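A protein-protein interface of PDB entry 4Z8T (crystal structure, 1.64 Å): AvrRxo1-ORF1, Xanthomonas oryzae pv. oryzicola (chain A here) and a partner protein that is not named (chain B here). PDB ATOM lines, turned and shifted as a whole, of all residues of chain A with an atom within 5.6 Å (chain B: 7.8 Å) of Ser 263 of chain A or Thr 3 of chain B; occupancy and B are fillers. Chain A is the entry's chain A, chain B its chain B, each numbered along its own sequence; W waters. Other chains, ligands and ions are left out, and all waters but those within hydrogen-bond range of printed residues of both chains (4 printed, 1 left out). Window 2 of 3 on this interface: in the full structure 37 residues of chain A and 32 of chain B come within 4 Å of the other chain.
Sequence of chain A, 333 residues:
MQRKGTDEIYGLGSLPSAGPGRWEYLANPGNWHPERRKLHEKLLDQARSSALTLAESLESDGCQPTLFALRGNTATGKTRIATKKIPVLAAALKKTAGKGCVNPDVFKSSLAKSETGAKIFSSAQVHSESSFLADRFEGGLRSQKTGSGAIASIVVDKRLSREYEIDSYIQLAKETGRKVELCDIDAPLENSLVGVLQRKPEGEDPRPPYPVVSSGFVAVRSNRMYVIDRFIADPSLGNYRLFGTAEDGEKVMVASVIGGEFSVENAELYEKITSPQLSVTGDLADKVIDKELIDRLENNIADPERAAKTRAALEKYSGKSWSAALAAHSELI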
ATOM      1  N   VAL A 254      25.687  24.876 -15.308  1.00  0.00           N
ATOM      2  CA  VAL A 254      27.025  24.929 -15.878  1.00  0.00           C
ATOM      3  C   VAL A 254      27.082  24.225 -17.235  1.00  0.00           C
ATOM      4  O   VAL A 254      27.658  24.747 -18.184  1.00  0.00           O
ATOM      5  CB  VAL A 254      28.044  24.313 -14.910  1.00  0.00           C
ATOM      6  CG1 VAL A 254      29.421  24.171 -15.591  1.00  0.00           C
ATOM      7  CG2 VAL A 254      28.179  25.196 -13.680  1.00  0.00           C
ATOM      8  N   ALA A 255      26.496  23.036 -17.317  1.00  0.00           N
ATOM      9  CA  ALA A 255      26.430  22.313 -18.596  1.00  0.00           C
ATOM     10  C   ALA A 255      25.184  21.445 -18.579  1.00  0.00           C
ATOM     11  O   ALA A 255      24.668  21.120 -17.516  1.00  0.00           O
ATOM     12  CB  ALA A 255      27.688  21.449 -18.814  1.00  0.00           C
ATOM     13  N   SER A 256      24.713  21.036 -19.750  1.00  0.00           N
ATOM     14  CA  SER A 256      23.485  20.256 -19.801  1.00  0.00           C
ATOM     15  C   SER A 256      23.362  19.433 -21.065  1.00  0.00           C
ATOM     16  O   SER A 256      23.874  19.809 -22.121  1.00  0.00           O
ATOM     17  CB  SER A 256      22.252  21.168 -19.666  1.00  0.00           C
ATOM     18  OG  SER A 256      22.171  22.108 -20.736  1.00  0.00           O
ATOM     19  N   VAL A 257      22.676  18.303 -20.960  1.00  0.00           N
ATOM     20  CA  VAL A 257      22.297  17.565 -22.159  1.00  0.00           C
ATOM     21  C   VAL A 257      20.812  17.293 -22.014  1.00  0.00           C
ATOM     22  O   VAL A 257      20.412  16.456 -21.211  1.00  0.00           O
ATOM     23  CB  VAL A 257      23.068  16.250 -22.307  1.00  0.00           C
ATOM     24  CG1 VAL A 257      22.788  15.651 -23.699  1.00  0.00           C
ATOM     25  CG2 VAL A 257      24.580  16.452 -22.115  1.00  0.00           C
ATOM     26  N   GLU A 261      20.461  17.700 -26.733  1.00  0.00           N
ATOM     27  CA  GLU A 261      21.211  18.901 -27.062  1.00  0.00           C
ATOM     28  C   GLU A 261      22.200  19.233 -25.948  1.00  0.00           C
ATOM     29  O   GLU A 261      21.799  19.382 -24.791  1.00  0.00           O
ATOM     30  CB  GLU A 261      20.245  20.063 -27.293  1.00  0.00           C
ATOM     31  CG  GLU A 261      20.906  21.356 -27.727  1.00  0.00           C
ATOM     32  CD  GLU A 261      20.067  22.147 -28.726  1.00  0.00           C
ATOM     33  OE1 GLU A 261      19.337  21.533 -29.536  1.00  0.00           O
ATOM     34  OE2 GLU A 261      20.140  23.395 -28.695  1.00  0.00           O
ATOM     35  N   PHE A 262      23.483  19.338 -26.297  1.00  0.00           N
ATOM     36  CA  PHE A 262      24.537  19.670 -25.330  1.00  0.00           C
ATOM     37  C   PHE A 262      24.894  21.153 -25.366  1.00  0.00           C
ATOM     38  O   PHE A 262      25.173  21.709 -26.428  1.00  0.00           O
ATOM     39  CB  PHE A 262      25.786  18.828 -25.606  1.00  0.00           C
ATOM     40  CG  PHE A 262      26.974  19.207 -24.765  1.00  0.00           C
ATOM     41  CD1 PHE A 262      26.950  19.052 -23.377  1.00  0.00           C
ATOM     42  CD2 PHE A 262      28.123  19.700 -25.353  1.00  0.00           C
ATOM     43  CE1 PHE A 262      28.047  19.381 -22.604  1.00  0.00           C
ATOM     44  CE2 PHE A 262      29.220  20.050 -24.576  1.00  0.00           C
ATOM     45  CZ  PHE A 262      29.190  19.885 -23.212  1.00  0.00           C
ATOM     46  N   SER A 263      24.861  21.800 -24.202  1.00  0.00           N
ATOM     47  CA  SER A 263      25.170  23.209 -24.089  1.00  0.00           C
ATOM     48  C   SER A 263      26.064  23.426 -22.891  1.00  0.00           C
ATOM     49  O   SER A 263      26.032  22.659 -21.941  1.00  0.00           O
ATOM     50  CB  SER A 263      23.885  24.005 -23.859  1.00  0.00           C
ATOM     51  OG  SER A 263      23.027  23.881 -24.973  1.00  0.00           O
ATOM     52  N   VAL A 264      26.866  24.475 -22.931  1.00  0.00           N
ATOM     53  CA  VAL A 264      27.678  24.826 -21.773  1.00  0.00           C
ATOM     54  C   VAL A 264      27.275  26.209 -21.330  1.00  0.00           C
ATOM     55  O   VAL A 264      27.711  27.202 -21.902  1.00  0.00           O
ATOM     56  CB  VAL A 264      29.179  24.789 -22.101  1.00  0.00           C
ATOM     57  CG1 VAL A 264      30.009  25.168 -20.856  1.00  0.00           C
ATOM     58  CG2 VAL A 264      29.567  23.404 -22.579  1.00  0.00           C
ATOM     59  N   GLU A 265      26.428  26.262 -20.309  1.00  0.00           N
ATOM     60  CA  GLU A 265      25.921  27.537 -19.809  1.00  0.00           C
ATOM     61  C   GLU A 265      26.963  28.382 -19.075  1.00  0.00           C
ATOM     62  O   GLU A 265      26.828  29.607 -19.017  1.00  0.00           O
ATOM     63  CB  GLU A 265      24.710  27.291 -18.910  1.00  0.00           C
ATOM     64  CG  GLU A 265      23.475  26.741 -19.651  1.00  0.00           C
ATOM     65  CD  GLU A 265      23.502  25.238 -19.847  1.00  0.00           C
ATOM     66  OE1 GLU A 265      22.592  24.709 -20.534  1.00  0.00           O
ATOM     67  OE2 GLU A 265      24.406  24.578 -19.295  1.00  0.00           O
ATOM     68  N   MET B   1      27.553  34.371 -18.202  1.00  0.00           N
ATOM     69  CA  MET B   1      28.159  34.556 -19.512  1.00  0.00           C
ATOM     70  C   MET B   1      27.341  33.891 -20.618  1.00  0.00           C
ATOM     71  O   MET B   1      26.398  33.147 -20.358  1.00  0.00           O
ATOM     72  CB  MET B   1      29.607  34.034 -19.522  1.00  0.00           C
ATOM     73  CG  MET B   1      29.757  32.538 -19.208  1.00  0.00           C
ATOM     74  SD  MET B   1      31.603  32.017 -18.836  1.00  0.00           S
ATOM     75  CE  MET B   1      32.238  31.879 -20.663  1.00  0.00           C
ATOM     76  N   LYS B   2      27.711  34.209 -21.852  1.00  0.00           N
ATOM     77  CA  LYS B   2      27.187  33.594 -23.065  1.00  0.00           C
ATOM     78  C   LYS B   2      27.233  32.061 -23.022  1.00  0.00           C
ATOM     79  O   LYS B   2      28.285  31.483 -22.753  1.00  0.00           O
ATOM     80  CB  LYS B   2      28.063  34.074 -24.217  1.00  0.00           C
ATOM     81  CG  LYS B   2      29.481  34.461 -23.764  1.00  0.00           C
ATOM     82  CD  LYS B   2      29.656  35.988 -23.608  1.00  0.00           C
ATOM     83  CE  LYS B   2      30.170  36.383 -22.218  1.00  0.00           C
ATOM     84  NZ  LYS B   2      31.548  35.884 -21.942  1.00  0.00           N
ATOM     85  N   THR B   3      26.106  31.409 -23.297  1.00  0.00           N
ATOM     86  CA  THR B   3      26.062  29.945 -23.347  1.00  0.00           C
ATOM     87  C   THR B   3      26.703  29.443 -24.641  1.00  0.00           C
ATOM     88  O   THR B   3      26.353  29.915 -25.722  1.00  0.00           O
ATOM     89  CB  THR B   3      24.607  29.419 -23.294  1.00  0.00           C
ATOM     90  OG1 THR B   3      24.033  29.689 -22.004  1.00  0.00           O
ATOM     91  CG2 THR B   3      24.570  27.929 -23.532  1.00  0.00           C
ATOM     92  N   LEU B   4      27.635  28.492 -24.541  1.00  0.00           N
ATOM     93  CA  LEU B   4      28.181  27.825 -25.729  1.00  0.00           C
ATOM     94  C   LEU B   4      27.183  26.779 -26.199  1.00  0.00           C
ATOM     95  O   LEU B   4      26.679  25.994 -25.394  1.00  0.00           O
ATOM     96  CB  LEU B   4      29.506  27.132 -25.415  1.00  0.00           C
ATOM     97  CG  LEU B   4      30.582  27.959 -24.732  1.00  0.00           C
ATOM     98  CD1 LEU B   4      31.842  27.132 -24.532  1.00  0.00           C
ATOM     99  CD2 LEU B   4      30.882  29.177 -25.558  1.00  0.00           C
ATOM    100  N   THR B   5      26.896  26.772 -27.500  1.00  0.00           N
ATOM    101  CA  THR B   5      25.883  25.892 -28.065  1.00  0.00           C
ATOM    102  C   THR B   5      26.490  25.152 -29.242  1.00  0.00           C
ATOM    103  O   THR B   5      27.578  25.520 -29.702  1.00  0.00           O
ATOM    104  CB  THR B   5      24.662  26.692 -28.578  1.00  0.00           C
ATOM    105  OG1 THR B   5      25.064  27.511 -29.681  1.00  0.00           O
ATOM    106  CG2 THR B   5      24.089  27.581 -27.474  1.00  0.00           C
ATOM    107  N   GLY B   6      25.798  24.117 -29.710  1.00  0.00           N
ATOM    108  CA  GLY B   6      26.178  23.426 -30.930  1.00  0.00           C
ATOM    109  C   GLY B   6      27.637  23.045 -31.054  1.00  0.00           C
ATOM    110  O   GLY B   6      28.230  22.438 -30.153  1.00  0.00           O
ATOM    111  N   ASP B   8      30.348  24.794 -31.017  1.00  0.00           N
ATOM    112  CA  ASP B   8      31.261  25.423 -30.061  1.00  0.00           C
ATOM    113  C   ASP B   8      31.243  24.668 -28.733  1.00  0.00           C
ATOM    114  O   ASP B   8      32.289  24.444 -28.123  1.00  0.00           O
ATOM    115  CB  ASP B   8      30.902  26.895 -29.810  1.00  0.00           C
ATOM    116  CG  ASP B   8      31.211  27.793 -30.997  1.00  0.00           C
ATOM    117  OD1 ASP B   8      32.116  27.461 -31.787  1.00  0.00           O
ATOM    118  OD2 ASP B   8      30.547  28.844 -31.120  1.00  0.00           O
ATOM    119  N   ALA B   9      30.057  24.270 -28.282  1.00  0.00           N
ATOM    120  CA  ALA B   9      29.971  23.515 -27.034  1.00  0.00           C
ATOM    121  C   ALA B   9      30.708  22.190 -27.175  1.00  0.00           C
ATOM    122  O   ALA B   9      31.478  21.804 -26.299  1.00  0.00           O
ATOM    123  CB  ALA B   9      28.517  23.279 -26.632  1.00  0.00           C
ATOM    124  N   LEU B  10      30.484  21.496 -28.291  1.00  0.00           N
ATOM    125  CA  LEU B  10      31.143  20.215 -28.505  1.00  0.00           C
ATOM    126  C   LEU B  10      32.659  20.334 -28.561  1.00  0.00           C
ATOM    127  O   LEU B  10      33.361  19.491 -28.014  1.00  0.00           O
ATOM    128  CB  LEU B  10      30.622  19.526 -29.768  1.00  0.00           C
ATOM    129  CG  LEU B  10      29.242  18.881 -29.647  1.00  0.00           C
ATOM    130  CD1 LEU B  10      28.755  18.408 -31.020  1.00  0.00           C
ATOM    131  CD2 LEU B  10      29.278  17.723 -28.672  1.00  0.00           C
HETATM  132  O   HOH W   1      29.499  29.481 -21.295  1.00  0.00           O
HETATM  133  O   HOH W   2      23.535  23.343 -28.085  1.00  0.00           O
HETATM  134  O   HOH W   3      24.660  31.536 -19.908  1.00  0.00           O
HETATM  135  O   HOH W   4      26.503  20.767 -28.678  1.00  0.00           O
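The backbone carbonyl oxygen (O) of Leu 4 of chain B lies within hydrogen-bond range of the backbone NH (N) of Val 264 of chain A (2.9 Å).
The backbone NH (N) of Ser 256 of chain A lies within hydrogen-bond range of the backbone carbonyl oxygen (O) of Ser 263 of chain A (3.0 Å).
OG of Ser 256 of chain A lies within hydrogen-bond range of OE1 of Glu 265 of chain A.
The backbone NH (N) of Ala 255 of chain A lies close to the side-chain carboxylate (OE2) of Glu 265 of chain A.
The backbone carbonyl oxygen (O) of Val 254 of chain A sits at hydrogen-bond distance from the backbone NH (N) of Glu 265 of chain A (2.9 Å).
Among the printed residues, merely in contact across the chains: Phe 262 of chain A with Ala 9 of chain B (3.3 Å), Ser 263 of chain A with Leu 4 of chain B (3.4 Å), Val 264 of chain A with Thr 3 of chain B (3.5 Å), Glu 265 of chain A with Thr 3 of chain B (3.6 Å), Glu 265 of chain A with Met 1 of chain B (3.8 Å) and Ser 263 of chain A with Thr 3 of chain B (3.997 Å).
Of the printed residues of chain B, Phe 262 of chain A touches Ala 9 (3.3 Å).
Of the printed residues of chain B, Ser 263 of chain A touches Thr 3 and Leu 4.
Printed residues of chain B within 4 Å of Val 264 of chain A: Thr 3 (3.5 Å) and Leu 4 (2.9 Å).
Of the printed residues of chain A, Thr 3 of chain B touches Ser 263 (3.997 Å), Val 264 (3.5 Å) and Glu 265 (3.6 Å).
The nearest printed residue of chain B that does not touch Ser 263 of chain A is Ala 9 of chain B (4.2 Å).
The nearest printed residue of chain A that does not touch Leu 4 of chain B is Phe 262 of chain A (4.7 Å).
Printed residues of chain B that touch a printed residue of chain A: Met 1, Thr 3, Leu 4 and Ala 9.
Hydrophobic or aromatic side chains of chain B that line the printed part of chain A: Leu 4 and Ala 9.
Of the 9 printed residues of chain A, 4 touch a printed residue of chain B.
Among the printed residues, 7 pairs touch across the chains.
Among the printed residues, no Asp or Glu carboxylate lies within 4 Å of a Lys or Arg side-chain nitrogen of the other chain.
Water W3 lies within hydrogen-bond range of O of Met 1 of chain B, OG1 of Thr 3 of chain B and O of Glu 265 of chain A.
Water W1 lies within hydrogen-bond range of O of Lys 2 of chain B (2.8 Å) and O of Val 264 of chain A (3.0 Å).
Water W4 bridges O of Phe 262 of chain A (2.8 Å) and O of Gly 6 of chain B (2.8 Å).
Water W2 lies within hydrogen-bond range of the backbone carbonyl oxygen (O) of Phe 262 of chain A, the backbone NH (N) of Gly 6 of chain B, the side-chain hydroxyl (OG) of Ser 263 of chain A and the side-chain carboxylate (OE2) of Glu 261 of chain A.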
